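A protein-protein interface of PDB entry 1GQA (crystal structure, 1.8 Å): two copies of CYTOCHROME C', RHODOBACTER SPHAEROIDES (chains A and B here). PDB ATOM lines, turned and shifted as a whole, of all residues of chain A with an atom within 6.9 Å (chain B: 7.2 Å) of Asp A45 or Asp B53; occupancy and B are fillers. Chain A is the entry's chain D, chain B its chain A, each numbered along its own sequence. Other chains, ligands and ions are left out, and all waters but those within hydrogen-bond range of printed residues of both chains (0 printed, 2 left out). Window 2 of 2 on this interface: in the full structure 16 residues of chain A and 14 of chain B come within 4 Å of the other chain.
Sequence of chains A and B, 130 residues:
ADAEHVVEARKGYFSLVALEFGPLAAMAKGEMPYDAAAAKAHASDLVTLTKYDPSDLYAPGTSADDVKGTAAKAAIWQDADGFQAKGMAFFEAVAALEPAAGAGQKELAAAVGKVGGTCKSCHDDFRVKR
The side-chain carboxylate (OD2) of Asp B53 is in hydrogen-bond range of the side-chain hydroxyl (OG) of Ser B55 (3.2 Å). ND1 of His A42 is in hydrogen-bond range of OE1 of Glu A20 (2.7 Å). The backbone carbonyl oxygen (O) of Ser A44 is in hydrogen-bond range of the side-chain hydroxyl (OG1) of Thr A48 (3.4 Å).
Hydrophobic or aromatic side chains of chain A that line the printed part of chain B: His A42 and Leu A49. Hydrophobic or aromatic side chains of chain B within 4 Å of the printed part of chain A: Tyr B52.
Thr B48 touches its own counterpart, Thr A48. 3 positions are printed for both chains. Of the 7 pairs that touch across the chains among the printed residues, 1 has its exchanged pair printed and touching as well.
Asp A45 touches Tyr B52 (OD2 to CD1, 3.4 Å). Thr A48 touches Thr B48. Leu A49 touches Tyr B52 (CD2 to CD1, 3.96 Å).
OH of Tyr B52 sits at hydrogen-bond distance from OE2 of Glu A20 (3.1 Å). The backbone NH (N) of Asp B53 is in hydrogen-bond range of the side-chain carboxylate (OD2) of Asp A45. A ring nitrogen (ND1) of His A42 sits close to the side-chain carboxylate (OD1) of Asp B56, at 3.0 Å. OE2 of Glu A20 sits close to OD1 of Asp B56 (2.9 Å).
Of the printed residues of chain B, His A42 touches Asp B56. Of the printed residues of chain B, Asp A45 touches Tyr B52 (3.4 Å) and Asp B53 (3.0 Å). Of the printed residues of chain B, Thr A48 touches Thr B48. Asp B53 touches one residue of chain A. The nearest residue of chain B that does not touch Asp A45 is Asp B56 (5.0 Å). The nearest printed residue of chain A that does not touch Asp B56 is Asp A45 (5.0 Å).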
ATOM      1  N   GLU A  20      -9.851 -23.340  -9.550  1.00  0.00           N
ATOM      2  CA  GLU A  20     -11.256 -23.513  -9.141  1.00  0.00           C
ATOM      3  C   GLU A  20     -12.143 -22.388  -9.644  1.00  0.00           C
ATOM      4  O   GLU A  20     -13.278 -22.609 -10.056  1.00  0.00           O
ATOM      5  CB  GLU A  20     -11.370 -23.638  -7.627  1.00  0.00           C
ATOM      6  CG  GLU A  20     -10.706 -24.883  -7.077  1.00  0.00           C
ATOM      7  CD  GLU A  20     -11.278 -26.155  -7.639  1.00  0.00           C
ATOM      8  OE1 GLU A  20     -12.479 -26.145  -7.969  1.00  0.00           O
ATOM      9  OE2 GLU A  20     -10.515 -27.171  -7.740  1.00  0.00           O
ATOM     10  N   LYS A  40     -21.334 -25.961  -7.987  1.00  0.00           N
ATOM     11  CA  LYS A  40     -21.381 -26.083  -6.550  1.00  0.00           C
ATOM     12  C   LYS A  40     -20.084 -26.651  -6.011  1.00  0.00           C
ATOM     13  O   LYS A  40     -19.553 -26.202  -4.991  1.00  0.00           O
ATOM     14  CB  LYS A  40     -22.526 -26.981  -6.101  1.00  0.00           C
ATOM     15  CG  LYS A  40     -22.653 -26.950  -4.601  1.00  0.00           C
ATOM     16  CD  LYS A  40     -24.144 -27.161  -4.199  1.00  0.00           C
ATOM     17  CE  LYS A  40     -25.077 -27.153  -5.454  1.00  0.00           C
ATOM     18  NZ  LYS A  40     -26.020 -28.317  -5.364  1.00  0.00           N
ATOM     19  N   ALA A  41     -19.566 -27.633  -6.727  1.00  0.00           N
ATOM     20  CA  ALA A  41     -18.319 -28.288  -6.370  1.00  0.00           C
ATOM     21  C   ALA A  41     -17.096 -27.313  -6.380  1.00  0.00           C
ATOM     22  O   ALA A  41     -16.280 -27.280  -5.419  1.00  0.00           O
ATOM     23  CB  ALA A  41     -18.095 -29.450  -7.305  1.00  0.00           C
ATOM     24  N   HIS A  42     -16.945 -26.559  -7.451  1.00  0.00           N
ATOM     25  CA  HIS A  42     -15.849 -25.623  -7.532  1.00  0.00           C
ATOM     26  C   HIS A  42     -16.015 -24.538  -6.451  1.00  0.00           C
ATOM     27  O   HIS A  42     -15.047 -24.161  -5.762  1.00  0.00           O
ATOM     28  CB  HIS A  42     -15.725 -24.984  -8.918  1.00  0.00           C
ATOM     29  CG  HIS A  42     -15.346 -25.955  -9.997  1.00  0.00           C
ATOM     30  ND1 HIS A  42     -14.164 -26.678  -9.979  1.00  0.00           N
ATOM     31  CD2 HIS A  42     -16.001 -26.337 -11.112  1.00  0.00           C
ATOM     32  CE1 HIS A  42     -14.117 -27.463 -11.040  1.00  0.00           C
ATOM     33  NE2 HIS A  42     -15.219 -27.275 -11.745  1.00  0.00           N
ATOM     34  N   ALA A  43     -17.221 -24.014  -6.315  1.00  0.00           N
ATOM     35  CA  ALA A  43     -17.467 -22.999  -5.290  1.00  0.00           C
ATOM     36  C   ALA A  43     -17.044 -23.474  -3.899  1.00  0.00           C
ATOM     37  O   ALA A  43     -16.355 -22.764  -3.159  1.00  0.00           O
ATOM     38  CB  ALA A  43     -18.918 -22.603  -5.284  1.00  0.00           C
ATOM     39  N   SER A  44     -17.483 -24.668  -3.515  1.00  0.00           N
ATOM     40  CA  SER A  44     -17.130 -25.199  -2.196  1.00  0.00           C
ATOM     41  C   SER A  44     -15.600 -25.388  -1.981  1.00  0.00           C
ATOM     42  O   SER A  44     -15.078 -25.055  -0.915  1.00  0.00           O
ATOM     43  CB  SER A  44     -17.988 -26.435  -1.859  1.00  0.00           C
ATOM     44  OG  SER A  44     -17.214 -27.516  -1.434  1.00  0.00           O
ATOM     45  N   ASP A  45     -14.875 -25.822  -3.012  1.00  0.00           N
ATOM     46  CA  ASP A  45     -13.417 -25.925  -2.873  1.00  0.00           C
ATOM     47  C   ASP A  45     -12.838 -24.552  -2.641  1.00  0.00           C
ATOM     48  O   ASP A  45     -11.882 -24.432  -1.894  1.00  0.00           O
ATOM     49  CB  ASP A  45     -12.752 -26.555  -4.076  1.00  0.00           C
ATOM     50  CG  ASP A  45     -12.443 -27.981  -3.854  1.00  0.00           C
ATOM     51  OD1 ASP A  45     -12.342 -28.704  -4.859  1.00  0.00           O
ATOM     52  OD2 ASP A  45     -12.263 -28.468  -2.690  1.00  0.00           O
ATOM     53  N   LEU A  46     -13.405 -23.526  -3.300  1.00  0.00           N
ATOM     54  CA  LEU A  46     -12.937 -22.136  -3.141  1.00  0.00           C
ATOM     55  C   LEU A  46     -13.145 -21.651  -1.732  1.00  0.00           C
ATOM     56  O   LEU A  46     -12.293 -20.982  -1.151  1.00  0.00           O
ATOM     57  CB  LEU A  46     -13.665 -21.182  -4.088  1.00  0.00           C
ATOM     58  CG  LEU A  46     -12.978 -20.877  -5.403  1.00  0.00           C
ATOM     59  CD1 LEU A  46     -13.896 -19.979  -6.206  1.00  0.00           C
ATOM     60  CD2 LEU A  46     -11.602 -20.203  -5.207  1.00  0.00           C
ATOM     61  N   VAL A  47     -14.293 -22.000  -1.175  1.00  0.00           N
ATOM     62  CA  VAL A  47     -14.570 -21.716   0.225  1.00  0.00           C
ATOM     63  C   VAL A  47     -13.495 -22.345   1.128  1.00  0.00           C
ATOM     64  O   VAL A  47     -12.974 -21.675   2.034  1.00  0.00           O
ATOM     65  CB  VAL A  47     -16.033 -22.136   0.618  1.00  0.00           C
ATOM     66  CG1 VAL A  47     -16.256 -22.078   2.141  1.00  0.00           C
ATOM     67  CG2 VAL A  47     -17.070 -21.237  -0.164  1.00  0.00           C
ATOM     68  N   THR A  48     -13.155 -23.613   0.889  1.00  0.00           N
ATOM     69  CA  THR A  48     -12.116 -24.249   1.673  1.00  0.00           C
ATOM     70  C   THR A  48     -10.782 -23.502   1.526  1.00  0.00           C
ATOM     71  O   THR A  48     -10.071 -23.369   2.488  1.00  0.00           O
ATOM     72  CB  THR A  48     -11.890 -25.688   1.246  1.00  0.00           C
ATOM     73  OG1 THR A  48     -13.082 -26.451   1.475  1.00  0.00           O
ATOM     74  CG2 THR A  48     -10.837 -26.341   2.158  1.00  0.00           C
ATOM     75  N   LEU A  49     -10.468 -23.011   0.328  1.00  0.00           N
ATOM     76  CA  LEU A  49      -9.200 -22.284   0.166  1.00  0.00           C
ATOM     77  C   LEU A  49      -9.180 -20.987   0.976  1.00  0.00           C
ATOM     78  O   LEU A  49      -8.166 -20.662   1.573  1.00  0.00           O
ATOM     79  CB  LEU A  49      -8.863 -22.006  -1.274  1.00  0.00           C
ATOM     80  CG  LEU A  49      -8.586 -23.206  -2.152  1.00  0.00           C
ATOM     81  CD1 LEU A  49      -8.500 -22.756  -3.608  1.00  0.00           C
ATOM     82  CD2 LEU A  49      -7.324 -23.908  -1.686  1.00  0.00           C
ATOM     83  N   THR A  50     -10.293 -20.271   1.019  1.00  0.00           N
ATOM     84  CA  THR A  50     -10.368 -19.030   1.785  1.00  0.00           C
ATOM     85  C   THR A  50     -10.253 -19.312   3.300  1.00  0.00           C
ATOM     86  O   THR A  50     -10.001 -18.398   4.079  1.00  0.00           O
ATOM     87  CB  THR A  50     -11.677 -18.248   1.497  1.00  0.00           C
ATOM     88  OG1 THR A  50     -12.802 -19.072   1.815  1.00  0.00           O
ATOM     89  CG2 THR A  50     -11.850 -17.914  -0.012  1.00  0.00           C
ATOM     90  N   VAL A  94     -16.558 -14.758  -1.717  1.00  0.00           N
ATOM     91  CA  VAL A  94     -16.523 -16.177  -1.985  1.00  0.00           C
ATOM     92  C   VAL A  94     -17.631 -16.871  -1.192  1.00  0.00           C
ATOM     93  O   VAL A  94     -18.264 -17.791  -1.707  1.00  0.00           O
ATOM     94  CB  VAL A  94     -15.153 -16.729  -1.620  1.00  0.00           C
ATOM     95  CG1 VAL A  94     -15.154 -18.297  -1.587  1.00  0.00           C
ATOM     96  CG2 VAL A  94     -14.114 -16.159  -2.581  1.00  0.00           C
ATOM     97  N   GLU A  98     -21.290 -19.438  -2.831  1.00  0.00           N
ATOM     98  CA  GLU A  98     -21.662 -20.824  -2.597  1.00  0.00           C
ATOM     99  C   GLU A  98     -23.132 -21.137  -2.897  1.00  0.00           C
ATOM    100  O   GLU A  98     -23.388 -21.927  -3.797  1.00  0.00           O
ATOM    101  CB  GLU A  98     -21.208 -21.320  -1.211  1.00  0.00           C
ATOM    102  CG  GLU A  98     -20.972 -22.813  -1.158  1.00  0.00           C
ATOM    103  CD  GLU A  98     -20.317 -23.224   0.152  1.00  0.00           C
ATOM    104  OE1 GLU A  98     -19.993 -24.441   0.292  1.00  0.00           O
ATOM    105  OE2 GLU A  98     -20.129 -22.329   1.033  1.00  0.00           O
ATOM    106  N   TYR B  13      -0.149 -27.440  -4.713  1.00  0.00           N
ATOM    107  CA  TYR B  13      -0.835 -28.138  -3.640  1.00  0.00           C
ATOM    108  C   TYR B  13       0.219 -28.818  -2.762  1.00  0.00           C
ATOM    109  O   TYR B  13       0.211 -28.639  -1.540  1.00  0.00           O
ATOM    110  CB  TYR B  13      -1.847 -29.167  -4.167  1.00  0.00           C
ATOM    111  CG  TYR B  13      -2.519 -29.990  -3.077  1.00  0.00           C
ATOM    112  CD1 TYR B  13      -3.554 -29.467  -2.322  1.00  0.00           C
ATOM    113  CD2 TYR B  13      -2.053 -31.273  -2.775  1.00  0.00           C
ATOM    114  CE1 TYR B  13      -4.157 -30.226  -1.334  1.00  0.00           C
ATOM    115  CE2 TYR B  13      -2.614 -32.028  -1.786  1.00  0.00           C
ATOM    116  CZ  TYR B  13      -3.667 -31.485  -1.055  1.00  0.00           C
ATOM    117  OH  TYR B  13      -4.241 -32.228  -0.053  1.00  0.00           O
ATOM    118  N   THR B  48      -6.854 -28.485   7.083  1.00  0.00           N
ATOM    119  CA  THR B  48      -7.593 -27.766   6.038  1.00  0.00           C
ATOM    120  C   THR B  48      -7.211 -28.238   4.657  1.00  0.00           C
ATOM    121  O   THR B  48      -8.077 -28.507   3.800  1.00  0.00           O
ATOM    122  CB  THR B  48      -7.376 -26.267   6.194  1.00  0.00           C
ATOM    123  OG1 THR B  48      -7.980 -25.844   7.423  1.00  0.00           O
ATOM    124  CG2 THR B  48      -8.156 -25.497   5.126  1.00  0.00           C
ATOM    125  N   LEU B  49      -5.918 -28.310   4.409  1.00  0.00           N
ATOM    126  CA  LEU B  49      -5.435 -28.836   3.163  1.00  0.00           C
ATOM    127  C   LEU B  49      -5.961 -30.216   2.822  1.00  0.00           C
ATOM    128  O   LEU B  49      -6.204 -30.480   1.656  1.00  0.00           O
ATOM    129  CB  LEU B  49      -3.929 -28.869   3.145  1.00  0.00           C
ATOM    130  CG  LEU B  49      -3.307 -27.496   3.220  1.00  0.00           C
ATOM    131  CD1 LEU B  49      -1.799 -27.624   2.962  1.00  0.00           C
ATOM    132  CD2 LEU B  49      -4.040 -26.496   2.265  1.00  0.00           C
ATOM    133  N   THR B  50      -6.113 -31.107   3.795  1.00  0.00           N
ATOM    134  CA  THR B  50      -6.575 -32.460   3.467  1.00  0.00           C
ATOM    135  C   THR B  50      -8.075 -32.425   3.221  1.00  0.00           C
ATOM    136  O   THR B  50      -8.629 -33.353   2.659  1.00  0.00           O
ATOM    137  CB  THR B  50      -6.218 -33.502   4.560  1.00  0.00           C
ATOM    138  OG1 THR B  50      -6.785 -33.090   5.813  1.00  0.00           O
ATOM    139  CG2 THR B  50      -4.692 -33.579   4.844  1.00  0.00           C
ATOM    140  N   LYS B  51      -8.736 -31.366   3.678  1.00  0.00           N
ATOM    141  CA  LYS B  51     -10.184 -31.253   3.472  1.00  0.00           C
ATOM    142  C   LYS B  51     -10.466 -30.858   2.026  1.00  0.00           C
ATOM    143  O   LYS B  51     -11.489 -31.213   1.506  1.00  0.00           O
ATOM    144  CB  LYS B  51     -10.834 -30.252   4.439  1.00  0.00           C
ATOM    145  CG  LYS B  51     -10.698 -30.610   5.959  1.00  0.00           C
ATOM    146  CD  LYS B  51     -11.980 -31.134   6.608  1.00  0.00           C
ATOM    147  CE  LYS B  51     -11.708 -31.604   8.028  1.00  0.00           C
ATOM    148  NZ  LYS B  51     -11.585 -30.440   8.950  1.00  0.00           N
ATOM    149  N   TYR B  52      -9.565 -30.110   1.405  1.00  0.00           N
ATOM    150  CA  TYR B  52      -9.679 -29.704   0.015  1.00  0.00           C
ATOM    151  C   TYR B  52      -9.786 -30.926  -0.878  1.00  0.00           C
ATOM    152  O   TYR B  52      -8.978 -31.842  -0.804  1.00  0.00           O
ATOM    153  CB  TYR B  52      -8.438 -28.897  -0.367  1.00  0.00           C
ATOM    154  CG  TYR B  52      -8.375 -28.496  -1.811  1.00  0.00           C
ATOM    155  CD1 TYR B  52      -9.088 -27.405  -2.282  1.00  0.00           C
ATOM    156  CD2 TYR B  52      -7.566 -29.168  -2.686  1.00  0.00           C
ATOM    157  CE1 TYR B  52      -9.031 -27.038  -3.616  1.00  0.00           C
ATOM    158  CE2 TYR B  52      -7.489 -28.820  -4.008  1.00  0.00           C
ATOM    159  CZ  TYR B  52      -8.222 -27.750  -4.475  1.00  0.00           C
ATOM    160  OH  TYR B  52      -8.126 -27.410  -5.815  1.00  0.00           O
ATOM    161  N   ASP B  53     -10.768 -30.940  -1.746  1.00  0.00           N
ATOM    162  CA  ASP B  53     -10.922 -32.072  -2.639  1.00  0.00           C
ATOM    163  C   ASP B  53     -10.036 -31.937  -3.867  1.00  0.00           C
ATOM    164  O   ASP B  53     -10.265 -31.060  -4.668  1.00  0.00           O
ATOM    165  CB  ASP B  53     -12.369 -32.156  -3.068  1.00  0.00           C
ATOM    166  CG  ASP B  53     -12.580 -33.200  -4.126  1.00  0.00           C
ATOM    167  OD1 ASP B  53     -12.519 -34.419  -3.839  1.00  0.00           O
ATOM    168  OD2 ASP B  53     -12.841 -32.875  -5.268  1.00  0.00           O
ATOM    169  N   PRO B  54      -9.030 -32.787  -4.027  1.00  0.00           N
ATOM    170  CA  PRO B  54      -8.049 -32.623  -5.126  1.00  0.00           C
ATOM    171  C   PRO B  54      -8.376 -33.205  -6.486  1.00  0.00           C
ATOM    172  O   PRO B  54      -7.464 -33.361  -7.299  1.00  0.00           O
ATOM    173  CB  PRO B  54      -6.810 -33.333  -4.611  1.00  0.00           C
ATOM    174  CG  PRO B  54      -7.214 -34.111  -3.377  1.00  0.00           C
ATOM    175  CD  PRO B  54      -8.714 -33.943  -3.171  1.00  0.00           C
ATOM    176  N   SER B  55      -9.636 -33.525  -6.720  1.00  0.00           N
ATOM    177  CA  SER B  55     -10.083 -34.081  -7.988  1.00  0.00           C
ATOM    178  C   SER B  55      -9.635 -33.331  -9.221  1.00  0.00           C
ATOM    179  O   SER B  55      -9.159 -33.948 -10.186  1.00  0.00           O
ATOM    180  CB  SER B  55     -11.590 -34.155  -7.975  1.00  0.00           C
ATOM    181  OG  SER B  55     -11.982 -35.291  -7.235  1.00  0.00           O
ATOM    182  N   ASP B  56      -9.803 -32.015  -9.227  1.00  0.00           N
ATOM    183  CA  ASP B  56      -9.409 -31.231 -10.398  1.00  0.00           C
ATOM    184  C   ASP B  56      -7.936 -31.316 -10.603  1.00  0.00           C
ATOM    185  O   ASP B  56      -7.423 -31.077 -11.707  1.00  0.00           O
ATOM    186  CB  ASP B  56      -9.836 -29.775 -10.255  1.00  0.00           C
ATOM    187  CG  ASP B  56     -11.331 -29.636 -10.271  1.00  0.00           C
ATOM    188  OD1 ASP B  56     -11.872 -28.612  -9.809  1.00  0.00           O
ATOM    189  OD2 ASP B  56     -12.032 -30.548 -10.735  1.00  0.00           O
ATOM    190  N   LEU B  57      -7.226 -31.694  -9.564  1.00  0.00           N
ATOM    191  CA  LEU B  57      -5.772 -31.754  -9.736  1.00  0.00           C
ATOM    192  C   LEU B  57      -5.350 -32.950 -10.572  1.00  0.00           C
ATOM    193  O   LEU B  57      -4.256 -33.014 -11.060  1.00  0.00           O
ATOM    194  CB  LEU B  57      -5.045 -31.838  -8.382  1.00  0.00           C
ATOM    195  CG  LEU B  57      -5.249 -30.670  -7.416  1.00  0.00           C
ATOM    196  CD1 LEU B  57      -4.538 -30.943  -6.045  1.00  0.00           C
ATOM    197  CD2 LEU B  57      -4.726 -29.436  -8.001  1.00  0.00           C
ATOM    198  N   GLN B  84      -6.626 -43.667  -3.867  1.00  0.00           N
ATOM    199  CA  GLN B  84      -7.476 -43.156  -2.772  1.00  0.00           C
ATOM    200  C   GLN B  84      -7.075 -43.742  -1.435  1.00  0.00           C
ATOM    201  O   GLN B  84      -7.151 -43.079  -0.418  1.00  0.00           O
ATOM    202  CB  GLN B  84      -8.977 -43.367  -3.033  1.00  0.00           C
ATOM    203  CG  GLN B  84      -9.682 -42.063  -3.449  1.00  0.00           C
ATOM    204  CD  GLN B  84      -9.845 -41.097  -2.286  1.00  0.00           C
ATOM    205  OE1 GLN B  84      -9.085 -40.117  -2.137  1.00  0.00           O
ATOM    206  NE2 GLN B  84     -10.838 -41.379  -1.439  1.00  0.00           N
